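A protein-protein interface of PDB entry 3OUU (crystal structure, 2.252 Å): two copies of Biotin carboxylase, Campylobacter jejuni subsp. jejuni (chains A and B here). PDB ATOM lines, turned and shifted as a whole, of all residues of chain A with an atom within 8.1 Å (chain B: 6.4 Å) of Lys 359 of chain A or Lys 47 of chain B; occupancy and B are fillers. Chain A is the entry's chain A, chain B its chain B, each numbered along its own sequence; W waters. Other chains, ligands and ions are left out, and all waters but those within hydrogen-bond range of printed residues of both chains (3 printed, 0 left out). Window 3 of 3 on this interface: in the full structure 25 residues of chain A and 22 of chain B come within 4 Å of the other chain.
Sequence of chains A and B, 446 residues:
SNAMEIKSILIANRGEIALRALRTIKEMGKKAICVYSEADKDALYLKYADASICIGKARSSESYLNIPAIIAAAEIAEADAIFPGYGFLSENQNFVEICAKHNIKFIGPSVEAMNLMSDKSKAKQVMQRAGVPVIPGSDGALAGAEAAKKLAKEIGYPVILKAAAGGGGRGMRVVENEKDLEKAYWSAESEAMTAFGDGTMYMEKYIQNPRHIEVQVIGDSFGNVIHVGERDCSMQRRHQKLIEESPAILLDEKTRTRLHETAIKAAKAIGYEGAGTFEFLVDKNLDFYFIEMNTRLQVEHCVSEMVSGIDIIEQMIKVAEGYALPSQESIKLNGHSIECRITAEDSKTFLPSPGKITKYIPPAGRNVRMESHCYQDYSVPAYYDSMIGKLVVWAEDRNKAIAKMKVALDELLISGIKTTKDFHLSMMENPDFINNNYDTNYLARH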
ATOM      1  N   LYS A 356       4.560 -15.463   1.958  1.00  0.00           N
ATOM      2  CA  LYS A 356       3.457 -14.608   1.560  1.00  0.00           C
ATOM      3  C   LYS A 356       3.398 -14.465   0.040  1.00  0.00           C
ATOM      4  O   LYS A 356       4.409 -14.247  -0.625  1.00  0.00           O
ATOM      5  CB  LYS A 356       3.545 -13.236   2.252  1.00  0.00           C
ATOM      6  CG  LYS A 356       2.497 -12.233   1.776  1.00  0.00           C
ATOM      7  CD  LYS A 356       2.629 -10.876   2.441  1.00  0.00           C
ATOM      8  CE  LYS A 356       1.944 -10.850   3.799  1.00  0.00           C
ATOM      9  NZ  LYS A 356       2.246  -9.582   4.535  1.00  0.00           N
ATOM     10  N   ILE A 357       2.204 -14.620  -0.511  1.00  0.00           N
ATOM     11  CA  ILE A 357       2.004 -14.434  -1.935  1.00  0.00           C
ATOM     12  C   ILE A 357       1.904 -12.946  -2.232  1.00  0.00           C
ATOM     13  O   ILE A 357       0.931 -12.316  -1.847  1.00  0.00           O
ATOM     14  CB  ILE A 357       0.695 -15.060  -2.365  1.00  0.00           C
ATOM     15  CG1 ILE A 357       0.767 -16.592  -2.263  1.00  0.00           C
ATOM     16  CG2 ILE A 357       0.331 -14.603  -3.789  1.00  0.00           C
ATOM     17  CD1 ILE A 357      -0.621 -17.221  -2.289  1.00  0.00           C
ATOM     18  N   THR A 358       2.896 -12.398  -2.922  1.00  0.00           N
ATOM     19  CA  THR A 358       2.972 -10.960  -3.174  1.00  0.00           C
ATOM     20  C   THR A 358       2.360 -10.616  -4.519  1.00  0.00           C
ATOM     21  O   THR A 358       2.110  -9.452  -4.814  1.00  0.00           O
ATOM     22  CB  THR A 358       4.422 -10.477  -3.187  1.00  0.00           C
ATOM     23  OG1 THR A 358       5.170 -11.319  -4.065  1.00  0.00           O
ATOM     24  CG2 THR A 358       5.045 -10.538  -1.770  1.00  0.00           C
ATOM     25  N   LYS A 359       2.126 -11.633  -5.342  1.00  0.00           N
ATOM     26  CA  LYS A 359       1.434 -11.417  -6.594  1.00  0.00           C
ATOM     27  C   LYS A 359       0.655 -12.678  -6.932  1.00  0.00           C
ATOM     28  O   LYS A 359       1.187 -13.788  -6.911  1.00  0.00           O
ATOM     29  CB  LYS A 359       2.412 -11.060  -7.700  1.00  0.00           C
ATOM     30  CG  LYS A 359       1.770 -10.726  -9.053  1.00  0.00           C
ATOM     31  CD  LYS A 359       2.881 -10.484 -10.073  1.00  0.00           C
ATOM     32  CE  LYS A 359       2.372  -9.914 -11.393  1.00  0.00           C
ATOM     33  NZ  LYS A 359       3.507  -9.479 -12.304  1.00  0.00           N
ATOM     34  N   TYR A 360      -0.628 -12.489  -7.203  1.00  0.00           N
ATOM     35  CA  TYR A 360      -1.507 -13.585  -7.515  1.00  0.00           C
ATOM     36  C   TYR A 360      -2.465 -13.176  -8.636  1.00  0.00           C
ATOM     37  O   TYR A 360      -3.353 -12.354  -8.456  1.00  0.00           O
ATOM     38  CB  TYR A 360      -2.285 -14.047  -6.270  1.00  0.00           C
ATOM     39  CG  TYR A 360      -3.123 -15.268  -6.566  1.00  0.00           C
ATOM     40  CD1 TYR A 360      -2.530 -16.511  -6.699  1.00  0.00           C
ATOM     41  CD2 TYR A 360      -4.493 -15.168  -6.772  1.00  0.00           C
ATOM     42  CE1 TYR A 360      -3.278 -17.633  -7.008  1.00  0.00           C
ATOM     43  CE2 TYR A 360      -5.254 -16.286  -7.074  1.00  0.00           C
ATOM     44  CZ  TYR A 360      -4.640 -17.518  -7.190  1.00  0.00           C
ATOM     45  OH  TYR A 360      -5.376 -18.640  -7.492  1.00  0.00           O
ATOM     46  N   ILE A 361      -2.262 -13.744  -9.804  1.00  0.00           N
ATOM     47  CA  ILE A 361      -3.182 -13.544 -10.902  1.00  0.00           C
ATOM     48  C   ILE A 361      -3.501 -14.912 -11.445  1.00  0.00           C
ATOM     49  O   ILE A 361      -2.627 -15.552 -12.017  1.00  0.00           O
ATOM     50  CB  ILE A 361      -2.556 -12.659 -11.996  1.00  0.00           C
ATOM     51  CG1 ILE A 361      -2.115 -11.324 -11.376  1.00  0.00           C
ATOM     52  CG2 ILE A 361      -3.555 -12.427 -13.121  1.00  0.00           C
ATOM     53  CD1 ILE A 361      -1.302 -10.430 -12.299  1.00  0.00           C
ATOM     54  N   PRO A 362      -4.740 -15.394 -11.220  1.00  0.00           N
ATOM     55  CA  PRO A 362      -5.123 -16.754 -11.654  1.00  0.00           C
ATOM     56  C   PRO A 362      -5.482 -16.814 -13.128  1.00  0.00           C
ATOM     57  O   PRO A 362      -5.851 -15.802 -13.705  1.00  0.00           O
ATOM     58  CB  PRO A 362      -6.366 -17.054 -10.825  1.00  0.00           C
ATOM     59  CG  PRO A 362      -6.994 -15.685 -10.588  1.00  0.00           C
ATOM     60  CD  PRO A 362      -5.815 -14.711 -10.472  1.00  0.00           C
ATOM     61  N   TYR A 375      -5.117 -15.493  -2.503  1.00  0.00           N
ATOM     62  CA  TYR A 375      -5.306 -14.160  -3.073  1.00  0.00           C
ATOM     63  C   TYR A 375      -4.025 -13.375  -2.787  1.00  0.00           C
ATOM     64  O   TYR A 375      -3.182 -13.827  -2.027  1.00  0.00           O
ATOM     65  CB  TYR A 375      -6.543 -13.488  -2.458  1.00  0.00           C
ATOM     66  CG  TYR A 375      -6.488 -13.469  -0.949  1.00  0.00           C
ATOM     67  CD1 TYR A 375      -5.924 -12.383  -0.271  1.00  0.00           C
ATOM     68  CD2 TYR A 375      -6.958 -14.549  -0.191  1.00  0.00           C
ATOM     69  CE1 TYR A 375      -5.840 -12.358   1.126  1.00  0.00           C
ATOM     70  CE2 TYR A 375      -6.879 -14.529   1.213  1.00  0.00           C
ATOM     71  CZ  TYR A 375      -6.324 -13.423   1.861  1.00  0.00           C
ATOM     72  OH  TYR A 375      -6.234 -13.374   3.239  1.00  0.00           O
ATOM     73  N   GLN A 376      -3.870 -12.212  -3.402  1.00  0.00           N
ATOM     74  CA  GLN A 376      -2.653 -11.456  -3.235  1.00  0.00           C
ATOM     75  C   GLN A 376      -2.572 -10.951  -1.798  1.00  0.00           C
ATOM     76  O   GLN A 376      -3.508 -10.310  -1.295  1.00  0.00           O
ATOM     77  CB  GLN A 376      -2.595 -10.315  -4.242  1.00  0.00           C
ATOM     78  CG  GLN A 376      -1.207  -9.733  -4.433  1.00  0.00           C
ATOM     79  CD  GLN A 376      -1.132  -8.830  -5.660  1.00  0.00           C
ATOM     80  OE1 GLN A 376      -1.497  -9.231  -6.772  1.00  0.00           O
ATOM     81  NE2 GLN A 376      -0.674  -7.604  -5.458  1.00  0.00           N
ATOM     82  N   ASP A 377      -1.456 -11.283  -1.150  1.00  0.00           N
ATOM     83  CA  ASP A 377      -1.154 -10.901   0.230  1.00  0.00           C
ATOM     84  C   ASP A 377      -1.457 -12.013   1.229  1.00  0.00           C
ATOM     85  O   ASP A 377      -1.191 -11.879   2.415  1.00  0.00           O
ATOM     86  CB  ASP A 377      -1.870  -9.609   0.645  1.00  0.00           C
ATOM     87  CG  ASP A 377      -1.451  -8.416  -0.192  1.00  0.00           C
ATOM     88  OD1 ASP A 377      -0.381  -8.492  -0.845  1.00  0.00           O
ATOM     89  OD2 ASP A 377      -2.196  -7.402  -0.192  1.00  0.00           O
ATOM     90  N   TYR A 378      -2.018 -13.105   0.744  1.00  0.00           N
ATOM     91  CA  TYR A 378      -2.325 -14.241   1.602  1.00  0.00           C
ATOM     92  C   TYR A 378      -1.039 -14.952   2.018  1.00  0.00           C
ATOM     93  O   TYR A 378      -0.102 -15.073   1.234  1.00  0.00           O
ATOM     94  CB  TYR A 378      -3.242 -15.213   0.843  1.00  0.00           C
ATOM     95  CG  TYR A 378      -3.634 -16.438   1.614  1.00  0.00           C
ATOM     96  CD1 TYR A 378      -4.326 -16.338   2.825  1.00  0.00           C
ATOM     97  CD2 TYR A 378      -3.347 -17.710   1.124  1.00  0.00           C
ATOM     98  CE1 TYR A 378      -4.710 -17.480   3.542  1.00  0.00           C
ATOM     99  CE2 TYR A 378      -3.725 -18.863   1.833  1.00  0.00           C
ATOM    100  CZ  TYR A 378      -4.412 -18.736   3.036  1.00  0.00           C
ATOM    101  OH  TYR A 378      -4.780 -19.873   3.722  1.00  0.00           O
ATOM    102  N   ASP A 410       0.609 -21.161 -18.161  1.00  0.00           N
ATOM    103  CA  ASP A 410       1.392 -19.996 -18.565  1.00  0.00           C
ATOM    104  C   ASP A 410       0.873 -18.686 -18.002  1.00  0.00           C
ATOM    105  O   ASP A 410       1.645 -17.761 -17.790  1.00  0.00           O
ATOM    106  CB  ASP A 410       1.441 -19.875 -20.090  1.00  0.00           C
ATOM    107  CG  ASP A 410       2.582 -20.692 -20.699  1.00  0.00           C
ATOM    108  OD1 ASP A 410       3.582 -20.920 -19.965  1.00  0.00           O
ATOM    109  OD2 ASP A 410       2.475 -21.124 -21.884  1.00  0.00           O
ATOM    110  N   GLU A 411      -0.434 -18.610 -17.772  1.00  0.00           N
ATOM    111  CA  GLU A 411      -1.074 -17.378 -17.326  1.00  0.00           C
ATOM    112  C   GLU A 411      -1.224 -17.301 -15.823  1.00  0.00           C
ATOM    113  O   GLU A 411      -1.564 -16.258 -15.281  1.00  0.00           O
ATOM    114  CB  GLU A 411      -2.433 -17.219 -17.993  1.00  0.00           C
ATOM    115  CG  GLU A 411      -2.301 -17.170 -19.502  1.00  0.00           C
ATOM    116  CD  GLU A 411      -3.630 -16.911 -20.252  1.00  0.00           C
ATOM    117  OE1 GLU A 411      -3.524 -16.517 -21.451  1.00  0.00           O
ATOM    118  OE2 GLU A 411      -4.734 -17.104 -19.647  1.00  0.00           O
ATOM    119  N   LEU A 412      -0.969 -18.405 -15.146  1.00  0.00           N
ATOM    120  CA  LEU A 412      -0.917 -18.396 -13.694  1.00  0.00           C
ATOM    121  C   LEU A 412       0.325 -17.609 -13.249  1.00  0.00           C
ATOM    122  O   LEU A 412       1.458 -18.020 -13.528  1.00  0.00           O
ATOM    123  CB  LEU A 412      -0.882 -19.827 -13.167  1.00  0.00           C
ATOM    124  CG  LEU A 412      -0.721 -19.918 -11.650  1.00  0.00           C
ATOM    125  CD1 LEU A 412      -1.764 -19.062 -10.932  1.00  0.00           C
ATOM    126  CD2 LEU A 412      -0.802 -21.370 -11.195  1.00  0.00           C
ATOM    127  N   LEU A 413       0.129 -16.456 -12.611  1.00  0.00           N
ATOM    128  CA  LEU A 413       1.286 -15.681 -12.149  1.00  0.00           C
ATOM    129  C   LEU A 413       1.259 -15.587 -10.635  1.00  0.00           C
ATOM    130  O   LEU A 413       0.352 -14.997 -10.053  1.00  0.00           O
ATOM    131  CB  LEU A 413       1.334 -14.275 -12.761  1.00  0.00           C
ATOM    132  CG  LEU A 413       1.364 -14.134 -14.295  1.00  0.00           C
ATOM    133  CD1 LEU A 413       1.197 -12.675 -14.721  1.00  0.00           C
ATOM    134  CD2 LEU A 413       2.639 -14.726 -14.882  1.00  0.00           C
ATOM    135  N   ILE A 414       2.243 -16.197  -9.998  1.00  0.00           N
ATOM    136  CA  ILE A 414       2.347 -16.168  -8.550  1.00  0.00           C
ATOM    137  C   ILE A 414       3.739 -15.734  -8.166  1.00  0.00           C
ATOM    138  O   ILE A 414       4.708 -16.189  -8.761  1.00  0.00           O
ATOM    139  CB  ILE A 414       2.115 -17.542  -7.968  1.00  0.00           C
ATOM    140  CG1 ILE A 414       0.635 -17.889  -8.057  1.00  0.00           C
ATOM    141  CG2 ILE A 414       2.620 -17.608  -6.529  1.00  0.00           C
ATOM    142  CD1 ILE A 414       0.298 -19.301  -7.608  1.00  0.00           C
ATOM    143  N   SER A 415       3.854 -14.845  -7.188  1.00  0.00           N
ATOM    144  CA  SER A 415       5.175 -14.467  -6.714  1.00  0.00           C
ATOM    145  C   SER A 415       5.238 -14.495  -5.198  1.00  0.00           C
ATOM    146  O   SER A 415       4.218 -14.305  -4.526  1.00  0.00           O
ATOM    147  CB  SER A 415       5.553 -13.087  -7.241  1.00  0.00           C
ATOM    148  OG  SER A 415       5.660 -13.134  -8.655  1.00  0.00           O
ATOM    149  N   GLY A 416       6.439 -14.736  -4.675  1.00  0.00           N
ATOM    150  CA  GLY A 416       6.696 -14.682  -3.245  1.00  0.00           C
ATOM    151  C   GLY A 416       6.907 -16.084  -2.714  1.00  0.00           C
ATOM    152  O   GLY A 416       7.435 -16.280  -1.621  1.00  0.00           O
ATOM    153  N   ILE A 417       6.481 -17.071  -3.494  1.00  0.00           N
ATOM    154  CA  ILE A 417       6.699 -18.462  -3.136  1.00  0.00           C
ATOM    155  C   ILE A 417       6.936 -19.243  -4.406  1.00  0.00           C
ATOM    156  O   ILE A 417       6.556 -18.795  -5.491  1.00  0.00           O
ATOM    157  CB  ILE A 417       5.498 -19.072  -2.358  1.00  0.00           C
ATOM    158  CG1 ILE A 417       4.183 -18.823  -3.090  1.00  0.00           C
ATOM    159  CG2 ILE A 417       5.410 -18.473  -0.970  1.00  0.00           C
ATOM    160  CD1 ILE A 417       3.017 -19.712  -2.642  1.00  0.00           C
ATOM    161  N   THR A 419       6.215 -22.509  -6.799  1.00  0.00           N
ATOM    162  CA  THR A 419       5.102 -23.438  -7.021  1.00  0.00           C
ATOM    163  C   THR A 419       5.493 -24.553  -7.949  1.00  0.00           C
ATOM    164  O   THR A 419       6.593 -24.548  -8.519  1.00  0.00           O
ATOM    165  CB  THR A 419       3.828 -22.755  -7.569  1.00  0.00           C
ATOM    166  OG1 THR A 419       4.041 -22.357  -8.918  1.00  0.00           O
ATOM    167  CG2 THR A 419       3.476 -21.536  -6.758  1.00  0.00           C
ATOM    168  N   LYS B  26      -3.614 -18.701 -28.796  1.00  0.00           N
ATOM    169  CA  LYS B  26      -2.535 -19.503 -28.271  1.00  0.00           C
ATOM    170  C   LYS B  26      -2.947 -20.968 -28.069  1.00  0.00           C
ATOM    171  O   LYS B  26      -2.137 -21.848 -28.306  1.00  0.00           O
ATOM    172  CB  LYS B  26      -2.001 -18.903 -26.977  1.00  0.00           C
ATOM    173  CG  LYS B  26      -1.406 -17.538 -27.186  1.00  0.00           C
ATOM    174  CD  LYS B  26      -0.579 -17.081 -25.985  1.00  0.00           C
ATOM    175  CE  LYS B  26       0.858 -17.576 -26.084  1.00  0.00           C
ATOM    176  NZ  LYS B  26       1.632 -17.262 -24.839  1.00  0.00           N
ATOM    177  N   ALA B  43      -0.910  -3.264 -19.530  1.00  0.00           N
ATOM    178  CA  ALA B  43      -1.973  -4.203 -19.864  1.00  0.00           C
ATOM    179  C   ALA B  43      -1.524  -5.637 -19.576  1.00  0.00           C
ATOM    180  O   ALA B  43      -0.432  -6.032 -19.958  1.00  0.00           O
ATOM    181  CB  ALA B  43      -2.377  -4.042 -21.338  1.00  0.00           C
ATOM    182  N   LEU B  44      -2.369  -6.411 -18.904  1.00  0.00           N
ATOM    183  CA  LEU B  44      -2.022  -7.786 -18.504  1.00  0.00           C
ATOM    184  C   LEU B  44      -1.615  -8.699 -19.686  1.00  0.00           C
ATOM    185  O   LEU B  44      -0.608  -9.392 -19.614  1.00  0.00           O
ATOM    186  CB  LEU B  44      -3.180  -8.419 -17.711  1.00  0.00           C
ATOM    187  CG  LEU B  44      -3.064  -9.904 -17.324  1.00  0.00           C
ATOM    188  CD1 LEU B  44      -1.822 -10.133 -16.450  1.00  0.00           C
ATOM    189  CD2 LEU B  44      -4.322 -10.381 -16.613  1.00  0.00           C
ATOM    190  N   TYR B  45      -2.392  -8.694 -20.770  1.00  0.00           N
ATOM    191  CA  TYR B  45      -2.147  -9.589 -21.904  1.00  0.00           C
ATOM    192  C   TYR B  45      -0.787  -9.361 -22.579  1.00  0.00           C
ATOM    193  O   TYR B  45      -0.291 -10.246 -23.277  1.00  0.00           O
ATOM    194  CB  TYR B  45      -3.273  -9.492 -22.940  1.00  0.00           C
ATOM    195  CG  TYR B  45      -3.656  -8.066 -23.262  1.00  0.00           C
ATOM    196  CD1 TYR B  45      -2.983  -7.356 -24.243  1.00  0.00           C
ATOM    197  CD2 TYR B  45      -4.668  -7.417 -22.551  1.00  0.00           C
ATOM    198  CE1 TYR B  45      -3.318  -6.033 -24.530  1.00  0.00           C
ATOM    199  CE2 TYR B  45      -5.008  -6.091 -22.829  1.00  0.00           C
ATOM    200  CZ  TYR B  45      -4.324  -5.411 -23.826  1.00  0.00           C
ATOM    201  OH  TYR B  45      -4.632  -4.110 -24.105  1.00  0.00           O
ATOM    202  N   LEU B  46      -0.186  -8.187 -22.378  1.00  0.00           N
ATOM    203  CA  LEU B  46       1.157  -7.943 -22.904  1.00  0.00           C
ATOM    204  C   LEU B  46       2.158  -8.947 -22.299  1.00  0.00           C
ATOM    205  O   LEU B  46       3.122  -9.343 -22.949  1.00  0.00           O
ATOM    206  CB  LEU B  46       1.615  -6.501 -22.653  1.00  0.00           C
ATOM    207  CG  LEU B  46       0.748  -5.379 -23.236  1.00  0.00           C
ATOM    208  CD1 LEU B  46       1.430  -4.029 -23.015  1.00  0.00           C
ATOM    209  CD2 LEU B  46       0.474  -5.617 -24.718  1.00  0.00           C
ATOM    210  N   LYS B  47       1.921  -9.367 -21.062  1.00  0.00           N
ATOM    211  CA  LYS B  47       2.739 -10.419 -20.480  1.00  0.00           C
ATOM    212  C   LYS B  47       2.570 -11.795 -21.151  1.00  0.00           C
ATOM    213  O   LYS B  47       3.458 -12.644 -21.067  1.00  0.00           O
ATOM    214  CB  LYS B  47       2.485 -10.531 -18.972  1.00  0.00           C
ATOM    215  CG  LYS B  47       3.561  -9.859 -18.129  1.00  0.00           C
ATOM    216  CD  LYS B  47       3.881 -10.681 -16.870  1.00  0.00           C
ATOM    217  CE  LYS B  47       5.124 -10.151 -16.124  1.00  0.00           C
ATOM    218  NZ  LYS B  47       5.442 -10.961 -14.899  1.00  0.00           N
ATOM    219  N   TYR B  48       1.446 -12.017 -21.825  1.00  0.00           N
ATOM    220  CA  TYR B  48       1.117 -13.345 -22.355  1.00  0.00           C
ATOM    221  C   TYR B  48       1.375 -13.479 -23.854  1.00  0.00           C
ATOM    222  O   TYR B  48       1.361 -14.579 -24.397  1.00  0.00           O
ATOM    223  CB  TYR B  48      -0.360 -13.659 -22.107  1.00  0.00           C
ATOM    224  CG  TYR B  48      -0.801 -13.690 -20.661  1.00  0.00           C
ATOM    225  CD1 TYR B  48       0.090 -13.986 -19.636  1.00  0.00           C
ATOM    226  CD2 TYR B  48      -2.130 -13.449 -20.325  1.00  0.00           C
ATOM    227  CE1 TYR B  48      -0.334 -14.034 -18.312  1.00  0.00           C
ATOM    228  CE2 TYR B  48      -2.569 -13.494 -19.014  1.00  0.00           C
ATOM    229  CZ  TYR B  48      -1.666 -13.784 -18.009  1.00  0.00           C
ATOM    230  OH  TYR B  48      -2.118 -13.819 -16.706  1.00  0.00           O
ATOM    231  N   ALA B  49       1.582 -12.363 -24.536  1.00  0.00           N
ATOM    232  CA  ALA B  49       1.618 -12.399 -25.991  1.00  0.00           C
ATOM    233  C   ALA B  49       2.980 -12.866 -26.440  1.00  0.00           C
ATOM    234  O   ALA B  49       3.950 -12.704 -25.704  1.00  0.00           O
ATOM    235  CB  ALA B  49       1.283 -11.015 -26.595  1.00  0.00           C
ATOM    236  N   SER B  52       4.780  -8.024 -28.471  1.00  0.00           N
ATOM    237  CA  SER B  52       3.993  -6.825 -28.194  1.00  0.00           C
ATOM    238  C   SER B  52       4.609  -5.615 -28.856  1.00  0.00           C
ATOM    239  O   SER B  52       5.794  -5.332 -28.682  1.00  0.00           O
ATOM    240  CB  SER B  52       3.908  -6.552 -26.693  1.00  0.00           C
ATOM    241  OG  SER B  52       2.916  -7.358 -26.088  1.00  0.00           O
ATOM    242  N   TYR B 375      -6.257  -6.551 -12.668  1.00  0.00           N
ATOM    243  CA  TYR B 375      -5.535  -7.252 -11.608  1.00  0.00           C
ATOM    244  C   TYR B 375      -5.247  -6.297 -10.444  1.00  0.00           C
ATOM    245  O   TYR B 375      -5.413  -5.094 -10.582  1.00  0.00           O
ATOM    246  CB  TYR B 375      -4.234  -7.869 -12.159  1.00  0.00           C
ATOM    247  CG  TYR B 375      -3.330  -6.868 -12.862  1.00  0.00           C
ATOM    248  CD1 TYR B 375      -2.317  -6.226 -12.165  1.00  0.00           C
ATOM    249  CD2 TYR B 375      -3.515  -6.535 -14.215  1.00  0.00           C
ATOM    250  CE1 TYR B 375      -1.491  -5.299 -12.772  1.00  0.00           C
ATOM    251  CE2 TYR B 375      -2.682  -5.612 -14.842  1.00  0.00           C
ATOM    252  CZ  TYR B 375      -1.665  -4.998 -14.100  1.00  0.00           C
ATOM    253  OH  TYR B 375      -0.820  -4.072 -14.661  1.00  0.00           O
HETATM  254  O   HOH W   1      -0.824 -17.602 -22.424  1.00  0.00           O
HETATM  255  O   HOH W   2       0.704 -19.517 -23.455  1.00  0.00           O
HETATM  256  O   HOH W   3      -4.919 -14.760 -16.443  1.00  0.00           O
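O of Glu 411 of chain A lies within hydrogen-bond range of OH of Tyr 48 of chain B (2.9 Å).
The backbone carbonyl oxygen of Leu 413 of chain A is in hydrogen-bond range of the backbone NH of Ile 361 of chain A, 2.9 Å away.
O of Lys 359 of chain A is in hydrogen-bond range of N of Ser 415 of chain A, at 2.9 Å.
The side-chain amino group of Lys 26 of chain B is in hydrogen-bond range of the backbone carbonyl oxygen of Tyr 48 of chain B, at 2.7 Å.
Among the printed residues, pairs that only touch across the chains: Lys 359 of chain A with Lys 47 of chain B (3.6 Å), Ile 361 of chain A with Tyr 375 of chain B (3.9 Å) and Leu 413 of chain A with Lys 47 of chain B (3.97 Å).
Lys 359 of chain A touches just one residue of chain B: Lys 47 (3.6 Å).
Lys 47 of chain B touches just these residues of chain A: Lys 359 (3.6 Å) and Leu 413 (3.97 Å).
Of the printed residues of chain A, Tyr 375 of chain B touches Ile 361.
Of the printed residues of chain B, Glu 411 of chain A touches Tyr 48.
Of the printed residues of chain A, Tyr 48 of chain B touches Glu 411 (2.9 Å).
Of the printed residues of chain B, Leu 413 of chain A touches Lys 47 (3.97 Å).
The nearest residue of chain A that does not touch Lys 47 of chain B is Asp 410 of chain A (6.3 Å).
The nearest printed residue of chain A that does not touch Tyr 375 of chain B is Tyr 360 of chain A (5.9 Å).
Printed residues of chain B that touch a printed residue of chain A: Lys 47, Tyr 48 and Tyr 375.
Among the printed residues, 4 pairs touch across the chains.
Position printed for both chains: 375.
Of the 4 pairs that touch across the chains among the printed residues, none has its exchanged pair printed and touching as well.
Water W2 bridges NZ of Lys 26 of chain B and OD2 of Asp 410 of chain A.
Water W3 lies within hydrogen-bond range of the side-chain hydroxyl of Tyr 48 of chain B and the backbone carbonyl oxygen of Pro 362 of chain A.
Water W1 bridges the side-chain carboxylate (OE1) of Glu 411 of chain A (3.1 Å) and the side-chain amino group (NZ) of Lys 26 of chain B (3.5 Å).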
